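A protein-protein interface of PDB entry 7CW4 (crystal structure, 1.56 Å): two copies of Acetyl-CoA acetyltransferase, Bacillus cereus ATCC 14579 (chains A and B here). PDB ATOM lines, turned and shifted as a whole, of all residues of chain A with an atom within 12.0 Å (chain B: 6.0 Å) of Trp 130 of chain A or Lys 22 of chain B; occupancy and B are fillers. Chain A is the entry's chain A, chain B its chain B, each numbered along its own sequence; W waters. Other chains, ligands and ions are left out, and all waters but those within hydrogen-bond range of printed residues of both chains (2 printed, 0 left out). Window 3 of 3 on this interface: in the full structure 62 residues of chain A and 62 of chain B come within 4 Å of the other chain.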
ATOM      1  N   ILE A 124      22.618  21.626 -12.817  1.00  0.00           N
ATOM      2  CA  ILE A 124      22.998  20.373 -13.500  1.00  0.00           C
ATOM      3  C   ILE A 124      24.506  20.292 -13.731  1.00  0.00           C
ATOM      4  O   ILE A 124      25.222  21.319 -13.790  1.00  0.00           O
ATOM      5  CB  ILE A 124      22.182  20.146 -14.782  1.00  0.00           C
ATOM      6  CG1 ILE A 124      22.653  21.032 -15.928  1.00  0.00           C
ATOM      7  CG2 ILE A 124      20.691  20.372 -14.481  1.00  0.00           C
ATOM      8  CD1 ILE A 124      22.152  20.561 -17.268  1.00  0.00           C
ATOM      9  N   LEU A 125      24.938  19.050 -13.900  1.00  0.00           N
ATOM     10  CA  LEU A 125      26.327  18.683 -14.226  1.00  0.00           C
ATOM     11  C   LEU A 125      26.291  17.872 -15.522  1.00  0.00           C
ATOM     12  O   LEU A 125      25.758  16.738 -15.485  1.00  0.00           O
ATOM     13  CB  LEU A 125      26.876  17.910 -13.038  1.00  0.00           C
ATOM     14  CG  LEU A 125      27.058  18.708 -11.740  1.00  0.00           C
ATOM     15  CD1 LEU A 125      27.318  17.737 -10.597  1.00  0.00           C
ATOM     16  CD2 LEU A 125      28.167  19.745 -11.836  1.00  0.00           C
ATOM     17  N   ARG A 126      26.795  18.384 -16.635  1.00  0.00           N
ATOM     18  CA  ARG A 126      26.737  17.642 -17.929  1.00  0.00           C
ATOM     19  C   ARG A 126      27.804  16.543 -18.027  1.00  0.00           C
ATOM     20  O   ARG A 126      27.584  15.555 -18.770  1.00  0.00           O
ATOM     21  CB  ARG A 126      26.931  18.601 -19.100  1.00  0.00           C
ATOM     22  CG  ARG A 126      25.833  19.633 -19.212  1.00  0.00           C
ATOM     23  CD  ARG A 126      26.047  20.419 -20.515  1.00  0.00           C
ATOM     24  NE  ARG A 126      25.274  21.637 -20.662  1.00  0.00           N
ATOM     25  CZ  ARG A 126      23.976  21.610 -20.909  1.00  0.00           C
ATOM     26  NH1 ARG A 126      23.376  20.449 -20.977  1.00  0.00           N
ATOM     27  NH2 ARG A 126      23.287  22.718 -21.077  1.00  0.00           N
ATOM     28  N   GLY A 127      28.891  16.650 -17.290  1.00  0.00           N
ATOM     29  CA  GLY A 127      30.033  15.702 -17.426  1.00  0.00           C
ATOM     30  C   GLY A 127      30.189  14.734 -16.278  1.00  0.00           C
ATOM     31  O   GLY A 127      31.167  13.947 -16.306  1.00  0.00           O
ATOM     32  N   ALA A 128      29.324  14.776 -15.280  1.00  0.00           N
ATOM     33  CA  ALA A 128      29.456  13.960 -14.053  1.00  0.00           C
ATOM     34  C   ALA A 128      29.205  12.481 -14.384  1.00  0.00           C
ATOM     35  O   ALA A 128      29.722  11.619 -13.619  1.00  0.00           O
ATOM     36  CB  ALA A 128      28.556  14.452 -12.960  1.00  0.00           C
ATOM     37  N   ARG A 129      28.424  12.187 -15.428  1.00  0.00           N
ATOM     38  CA  ARG A 129      28.042  10.785 -15.738  1.00  0.00           C
ATOM     39  C   ARG A 129      29.245  10.016 -16.260  1.00  0.00           C
ATOM     40  O   ARG A 129      29.488   8.914 -15.741  1.00  0.00           O
ATOM     41  CB  ARG A 129      26.887  10.725 -16.733  1.00  0.00           C
ATOM     42  CG  ARG A 129      26.425   9.301 -17.013  1.00  0.00           C
ATOM     43  CD  ARG A 129      25.253   9.210 -17.947  1.00  0.00           C
ATOM     44  NE  ARG A 129      24.136   9.978 -17.436  1.00  0.00           N
ATOM     45  CZ  ARG A 129      23.295   9.597 -16.485  1.00  0.00           C
ATOM     46  NH1 ARG A 129      23.443   8.422 -15.899  1.00  0.00           N
ATOM     47  NH2 ARG A 129      22.283  10.361 -16.119  1.00  0.00           N
ATOM     48  N   TRP A 130      29.914  10.555 -17.272  1.00  0.00           N
ATOM     49  CA  TRP A 130      31.040   9.861 -17.938  1.00  0.00           C
ATOM     50  C   TRP A 130      32.388  10.443 -17.496  1.00  0.00           C
ATOM     51  O   TRP A 130      33.415   9.807 -17.816  1.00  0.00           O
ATOM     52  CB  TRP A 130      30.862   9.887 -19.454  1.00  0.00           C
ATOM     53  CG  TRP A 130      29.572   9.230 -19.855  1.00  0.00           C
ATOM     54  CD1 TRP A 130      28.489   9.863 -20.414  1.00  0.00           C
ATOM     55  CD2 TRP A 130      29.194   7.849 -19.708  1.00  0.00           C
ATOM     56  NE1 TRP A 130      27.500   8.953 -20.654  1.00  0.00           N
ATOM     57  CE2 TRP A 130      27.851   7.734 -20.152  1.00  0.00           C
ATOM     58  CE3 TRP A 130      29.815   6.709 -19.170  1.00  0.00           C
ATOM     59  CZ2 TRP A 130      27.191   6.509 -20.206  1.00  0.00           C
ATOM     60  CZ3 TRP A 130      29.133   5.506 -19.167  1.00  0.00           C
ATOM     61  CH2 TRP A 130      27.833   5.416 -19.671  1.00  0.00           C
ATOM     62  N   GLY A 131      32.373  11.519 -16.709  1.00  0.00           N
ATOM     63  CA  GLY A 131      33.587  12.063 -16.077  1.00  0.00           C
ATOM     64  C   GLY A 131      34.112  13.324 -16.744  1.00  0.00           C
ATOM     65  O   GLY A 131      34.212  13.372 -17.978  1.00  0.00           O
ATOM     66  N   TYR A 132      34.549  14.291 -15.950  1.00  0.00           N
ATOM     67  CA  TYR A 132      35.232  15.522 -16.414  1.00  0.00           C
ATOM     68  C   TYR A 132      36.681  15.194 -16.797  1.00  0.00           C
ATOM     69  O   TYR A 132      37.274  16.015 -17.528  1.00  0.00           O
ATOM     70  CB  TYR A 132      35.057  16.591 -15.338  1.00  0.00           C
ATOM     71  CG  TYR A 132      33.628  17.096 -15.228  1.00  0.00           C
ATOM     72  CD1 TYR A 132      33.080  17.884 -16.235  1.00  0.00           C
ATOM     73  CD2 TYR A 132      32.865  16.857 -14.105  1.00  0.00           C
ATOM     74  CE1 TYR A 132      31.783  18.389 -16.139  1.00  0.00           C
ATOM     75  CE2 TYR A 132      31.581  17.349 -14.002  1.00  0.00           C
ATOM     76  CZ  TYR A 132      31.031  18.091 -15.025  1.00  0.00           C
ATOM     77  OH  TYR A 132      29.741  18.576 -14.974  1.00  0.00           O
ATOM     78  N   ARG A 133      37.249  14.164 -16.169  1.00  0.00           N
ATOM     79  CA  ARG A 133      38.655  13.699 -16.349  1.00  0.00           C
ATOM     80  C   ARG A 133      39.638  14.714 -15.741  1.00  0.00           C
ATOM     81  O   ARG A 133      40.304  14.394 -14.733  1.00  0.00           O
ATOM     82  CB  ARG A 133      38.946  13.458 -17.842  1.00  0.00           C
ATOM     83  CG  ARG A 133      40.359  12.935 -18.058  1.00  0.00           C
ATOM     84  CD  ARG A 133      40.641  12.300 -19.422  1.00  0.00           C
ATOM     85  NE  ARG A 133      41.828  11.454 -19.215  1.00  0.00           N
ATOM     86  CZ  ARG A 133      43.067  11.910 -19.202  1.00  0.00           C
ATOM     87  NH1 ARG A 133      43.296  13.194 -19.437  1.00  0.00           N
ATOM     88  NH2 ARG A 133      44.075  11.074 -18.989  1.00  0.00           N
ATOM     89  N   MET A 134      39.772  15.900 -16.324  1.00  0.00           N
ATOM     90  CA  MET A 134      40.604  16.936 -15.697  1.00  0.00           C
ATOM     91  C   MET A 134      40.195  18.317 -16.191  1.00  0.00           C
ATOM     92  O   MET A 134      39.652  18.450 -17.331  1.00  0.00           O
ATOM     93  CB  MET A 134      42.098  16.693 -15.921  1.00  0.00           C
ATOM     94  CG  MET A 134      42.626  17.014 -17.268  1.00  0.00           C
ATOM     95  SD  MET A 134      44.502  16.782 -17.246  1.00  0.00           S
ATOM     96  CE  MET A 134      44.877  17.312 -15.589  1.00  0.00           C
ATOM     97  N   GLY A 135      40.456  19.306 -15.362  1.00  0.00           N
ATOM     98  CA  GLY A 135      40.168  20.700 -15.686  1.00  0.00           C
ATOM     99  C   GLY A 135      38.831  21.104 -15.102  1.00  0.00           C
ATOM    100  O   GLY A 135      37.971  20.232 -14.885  1.00  0.00           O
ATOM    101  N   ASN A 137      35.112  22.863 -14.935  1.00  0.00           N
ATOM    102  CA  ASN A 137      33.968  22.822 -15.854  1.00  0.00           C
ATOM    103  C   ASN A 137      32.844  23.627 -15.203  1.00  0.00           C
ATOM    104  O   ASN A 137      33.132  24.441 -14.316  1.00  0.00           O
ATOM    105  CB  ASN A 137      33.580  21.393 -16.185  1.00  0.00           C
ATOM    106  CG  ASN A 137      33.074  21.299 -17.598  1.00  0.00           C
ATOM    107  OD1 ASN A 137      32.010  21.859 -17.914  1.00  0.00           O
ATOM    108  ND2 ASN A 137      33.802  20.559 -18.413  1.00  0.00           N
ATOM    109  N   LYS B  16      22.853   1.033 -27.181  1.00  0.00           N
ATOM    110  CA  LYS B  16      22.972   0.689 -25.761  1.00  0.00           C
ATOM    111  C   LYS B  16      23.425   1.929 -24.973  1.00  0.00           C
ATOM    112  O   LYS B  16      24.058   2.854 -25.530  1.00  0.00           O
ATOM    113  CB  LYS B  16      23.954  -0.458 -25.486  1.00  0.00           C
ATOM    114  CG  LYS B  16      23.558  -1.788 -26.109  1.00  0.00           C
ATOM    115  CD  LYS B  16      24.489  -2.914 -25.783  1.00  0.00           C
ATOM    116  CE  LYS B  16      24.292  -3.378 -24.359  1.00  0.00           C
ATOM    117  NZ  LYS B  16      25.137  -4.562 -24.075  1.00  0.00           N
ATOM    118  N   PHE B  17      23.131   1.936 -23.695  1.00  0.00           N
ATOM    119  CA  PHE B  17      23.600   2.977 -22.757  1.00  0.00           C
ATOM    120  C   PHE B  17      25.110   3.051 -22.798  1.00  0.00           C
ATOM    121  O   PHE B  17      25.740   2.028 -22.566  1.00  0.00           O
ATOM    122  CB  PHE B  17      23.104   2.629 -21.364  1.00  0.00           C
ATOM    123  CG  PHE B  17      23.446   3.672 -20.331  1.00  0.00           C
ATOM    124  CD1 PHE B  17      22.746   4.858 -20.295  1.00  0.00           C
ATOM    125  CD2 PHE B  17      24.391   3.422 -19.383  1.00  0.00           C
ATOM    126  CE1 PHE B  17      23.005   5.809 -19.318  1.00  0.00           C
ATOM    127  CE2 PHE B  17      24.668   4.377 -18.413  1.00  0.00           C
ATOM    128  CZ  PHE B  17      23.968   5.560 -18.389  1.00  0.00           C
ATOM    129  N   GLY B  18      25.660   4.223 -23.120  1.00  0.00           N
ATOM    130  CA  GLY B  18      27.126   4.398 -23.268  1.00  0.00           C
ATOM    131  C   GLY B  18      27.698   3.711 -24.490  1.00  0.00           C
ATOM    132  O   GLY B  18      28.921   3.460 -24.513  1.00  0.00           O
ATOM    133  N   GLY B  19      26.858   3.360 -25.448  1.00  0.00           N
ATOM    134  CA  GLY B  19      27.219   2.541 -26.604  1.00  0.00           C
ATOM    135  C   GLY B  19      27.370   3.320 -27.871  1.00  0.00           C
ATOM    136  O   GLY B  19      28.015   4.364 -27.896  1.00  0.00           O
ATOM    137  N   SER B  20      26.871   2.713 -28.936  1.00  0.00           N
ATOM    138  CA  SER B  20      27.157   3.117 -30.318  1.00  0.00           C
ATOM    139  C   SER B  20      26.728   4.552 -30.574  1.00  0.00           C
ATOM    140  O   SER B  20      27.348   5.159 -31.460  1.00  0.00           O
ATOM    141  CB  SER B  20      26.536   2.128 -31.295  1.00  0.00           C
ATOM    142  OG  SER B  20      25.129   2.097 -31.177  1.00  0.00           O
ATOM    143  N   LEU B  21      25.638   5.037 -29.951  1.00  0.00           N
ATOM    144  CA  LEU B  21      25.111   6.400 -30.218  1.00  0.00           C
ATOM    145  C   LEU B  21      25.436   7.353 -29.062  1.00  0.00           C
ATOM    146  O   LEU B  21      24.828   8.455 -29.018  1.00  0.00           O
ATOM    147  CB  LEU B  21      23.611   6.352 -30.496  1.00  0.00           C
ATOM    148  CG  LEU B  21      23.185   5.401 -31.609  1.00  0.00           C
ATOM    149  CD1 LEU B  21      21.648   5.330 -31.728  1.00  0.00           C
ATOM    150  CD2 LEU B  21      23.776   5.829 -32.957  1.00  0.00           C
ATOM    151  N   LYS B  22      26.354   6.996 -28.175  1.00  0.00           N
ATOM    152  CA  LYS B  22      26.604   7.793 -26.950  1.00  0.00           C
ATOM    153  C   LYS B  22      27.022   9.227 -27.316  1.00  0.00           C
ATOM    154  O   LYS B  22      26.766  10.145 -26.504  1.00  0.00           O
ATOM    155  CB  LYS B  22      27.632   7.061 -26.097  1.00  0.00           C
ATOM    156  CG  LYS B  22      29.078   7.253 -26.487  1.00  0.00           C
ATOM    157  CD  LYS B  22      30.027   7.068 -25.266  1.00  0.00           C
ATOM    158  CE  LYS B  22      29.470   7.652 -23.981  1.00  0.00           C
ATOM    159  NZ  LYS B  22      30.529   8.145 -23.079  1.00  0.00           N
ATOM    160  N   ASP B  23      27.667   9.455 -28.463  1.00  0.00           N
ATOM    161  CA  ASP B  23      28.182  10.809 -28.808  1.00  0.00           C
ATOM    162  C   ASP B  23      27.175  11.572 -29.665  1.00  0.00           C
ATOM    163  O   ASP B  23      27.555  12.640 -30.199  1.00  0.00           O
ATOM    164  CB  ASP B  23      29.539  10.725 -29.496  1.00  0.00           C
ATOM    165  CG  ASP B  23      30.619  10.163 -28.589  1.00  0.00           C
ATOM    166  OD1 ASP B  23      30.638  10.480 -27.392  1.00  0.00           O
ATOM    167  OD2 ASP B  23      31.355   9.338 -29.080  1.00  0.00           O
ATOM    168  N   VAL B  24      25.924  11.106 -29.753  1.00  0.00           N
ATOM    169  CA  VAL B  24      24.872  11.754 -30.575  1.00  0.00           C
ATOM    170  C   VAL B  24      23.784  12.294 -29.639  1.00  0.00           C
ATOM    171  O   VAL B  24      23.222  11.545 -28.827  1.00  0.00           O
ATOM    172  CB  VAL B  24      24.253  10.789 -31.600  1.00  0.00           C
ATOM    173  CG1 VAL B  24      23.359  11.526 -32.567  1.00  0.00           C
ATOM    174  CG2 VAL B  24      25.356  10.015 -32.296  1.00  0.00           C
ATOM    175  N   LYS B  25      23.490  13.582 -29.729  1.00  0.00           N
ATOM    176  CA  LYS B  25      22.432  14.197 -28.872  1.00  0.00           C
ATOM    177  C   LYS B  25      21.072  13.628 -29.253  1.00  0.00           C
ATOM    178  O   LYS B  25      20.830  13.278 -30.423  1.00  0.00           O
ATOM    179  CB  LYS B  25      22.462  15.723 -28.989  1.00  0.00           C
ATOM    180  CG  LYS B  25      23.760  16.369 -28.554  1.00  0.00           C
ATOM    181  CD  LYS B  25      23.627  17.828 -28.293  1.00  0.00           C
ATOM    182  CE  LYS B  25      22.816  18.523 -29.357  1.00  0.00           C
ATOM    183  NZ  LYS B  25      22.845  19.998 -29.194  1.00  0.00           N
ATOM    184  N   SER B 117      18.176  10.303 -25.598  1.00  0.00           N
ATOM    185  CA  SER B 117      19.592   9.915 -25.403  1.00  0.00           C
ATOM    186  C   SER B 117      19.797   9.690 -23.916  1.00  0.00           C
ATOM    187  O   SER B 117      20.153  10.609 -23.190  1.00  0.00           O
ATOM    188  CB  SER B 117      20.551  10.923 -25.970  1.00  0.00           C
ATOM    189  OG  SER B 117      21.867  10.466 -25.678  1.00  0.00           O
ATOM    190  N   SER B 119      21.996   8.014 -22.603  1.00  0.00           N
ATOM    191  CA  SER B 119      23.470   8.122 -22.416  1.00  0.00           C
ATOM    192  C   SER B 119      23.866   9.539 -21.951  1.00  0.00           C
ATOM    193  O   SER B 119      24.871   9.689 -21.237  1.00  0.00           O
ATOM    194  CB  SER B 119      24.188   7.789 -23.695  1.00  0.00           C
ATOM    195  OG  SER B 119      24.071   6.406 -24.007  1.00  0.00           O
ATOM    196  N   ASN B 120      23.156  10.558 -22.418  1.00  0.00           N
ATOM    197  CA  ASN B 120      23.568  11.963 -22.255  1.00  0.00           C
ATOM    198  C   ASN B 120      22.749  12.706 -21.208  1.00  0.00           C
ATOM    199  O   ASN B 120      23.022  13.926 -21.019  1.00  0.00           O
ATOM    200  CB  ASN B 120      23.619  12.693 -23.583  1.00  0.00           C
ATOM    201  CG  ASN B 120      24.773  12.200 -24.433  1.00  0.00           C
ATOM    202  OD1 ASN B 120      25.916  12.165 -23.974  1.00  0.00           O
ATOM    203  ND2 ASN B 120      24.464  11.605 -25.578  1.00  0.00           N
ATOM    204  N   ASP B 252      19.350   4.663 -26.333  1.00  0.00           N
ATOM    205  CA  ASP B 252      19.324   5.870 -27.185  1.00  0.00           C
ATOM    206  C   ASP B 252      18.651   5.586 -28.526  1.00  0.00           C
ATOM    207  O   ASP B 252      18.922   4.529 -29.075  1.00  0.00           O
ATOM    208  CB  ASP B 252      20.760   6.304 -27.480  1.00  0.00           C
ATOM    209  CG  ASP B 252      21.586   6.588 -26.237  1.00  0.00           C
ATOM    210  OD1 ASP B 252      20.995   6.975 -25.229  1.00  0.00           O
ATOM    211  OD2 ASP B 252      22.850   6.410 -26.296  1.00  0.00           O
HETATM  212  O   HOH W   1      24.614  15.781 -19.819  1.00  0.00           O
HETATM  213  O   HOH W   2      25.761  12.969 -19.082  1.00  0.00           O
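No position is printed for both chains.
NE1 of Trp 130 of chain A lies within hydrogen-bond range of O of Ser 119 of chain B (2.8 Å).
The backbone NH of Gly 18 of chain B sits at hydrogen-bond distance from the side-chain hydroxyl of Ser 119 of chain B, at 2.8 Å.
The backbone carbonyl oxygen of Lys 22 of chain B lies within hydrogen-bond range of the side-chain amide nitrogen of Asn 120 of chain B, 2.9 Å away.
OD2 of Asp 252 of chain B sits at hydrogen-bond distance from OG of Ser 119 of chain B (2.6 Å).
Ile 124 of chain A touches none of the printed residues of chain B.
Printed residues of chain B within 4 Å of Arg 129 of chain A: Phe 17 (3.8 Å) and Ser 119 (3.3 Å).
Of chain B, only Phe 17 (3.6 Å), Gly 18 (3.7 Å), Lys 22 (3.5 Å) and Ser 119 (2.8 Å) come within 4 Å of Trp 130 of chain A.
Of chain A, only Arg 129 (3.8 Å) and Trp 130 (3.6 Å) come within 4 Å of Phe 17 of chain B.
Gly 18 of chain B touches just one residue of chain A: Trp 130 (3.7 Å).
No residue of chain A comes within 4 Å of Gly 19 of chain B.
No residue of chain A comes within 4 Å of Ser 20 of chain B.
No residue of chain A comes within 4 Å of Leu 21 of chain B.
Lys 22 of chain B touches just one residue of chain A: Trp 130 (3.5 Å).
Asp 23 of chain B touches none of the printed residues of chain A.
No residue of chain A comes within 4 Å of Val 24 of chain B.
Ser 117 of chain B touches none of the printed residues of chain A.
Of the printed residues of chain A, Ser 119 of chain B touches Arg 129 and Trp 130.
No residue of chain A comes within 4 Å of Asn 120 of chain B.
The nearest residue of chain B that does not touch Trp 130 of chain A is Asn 120 of chain B (4.9 Å).
The nearest residue of chain A that does not touch Lys 22 of chain B is Arg 129 of chain A (7.2 Å).
Arg 129 of chain A touches Phe 17 of chain B (NH1 to CZ, 3.8 Å).
O of Ser 119 of chain B touches CD of Arg 129 of chain A (3.3 Å).
CE2 of Phe 17 of chain B touches CH2 of Trp 130 of chain A, 3.6 Å away.
Trp 130 of chain A touches Gly 18 of chain B.
NZ of Lys 22 of chain B touches CG of Trp 130 of chain A (3.5 Å).
Of the 13 printed residues of chain A, 2 touch a printed residue of chain B.
Hydrophobic or aromatic side chains of chain A within 4 Å of the printed part of chain B: Trp 130.
Of the 14 printed residues of chain B, 4 touch a printed residue of chain A.
Water W1 bridges the backbone carbonyl oxygen (O) of Asn 120 of chain B (2.7 Å) and the backbone carbonyl oxygen (O) of Arg 126 of chain A (3.2 Å).
Water W2 lies within hydrogen-bond range of the backbone carbonyl oxygen (O) of Arg 126 of chain A (3.2 Å) and the backbone carbonyl oxygen (O) of Asn 120 of chain B (3.5 Å).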
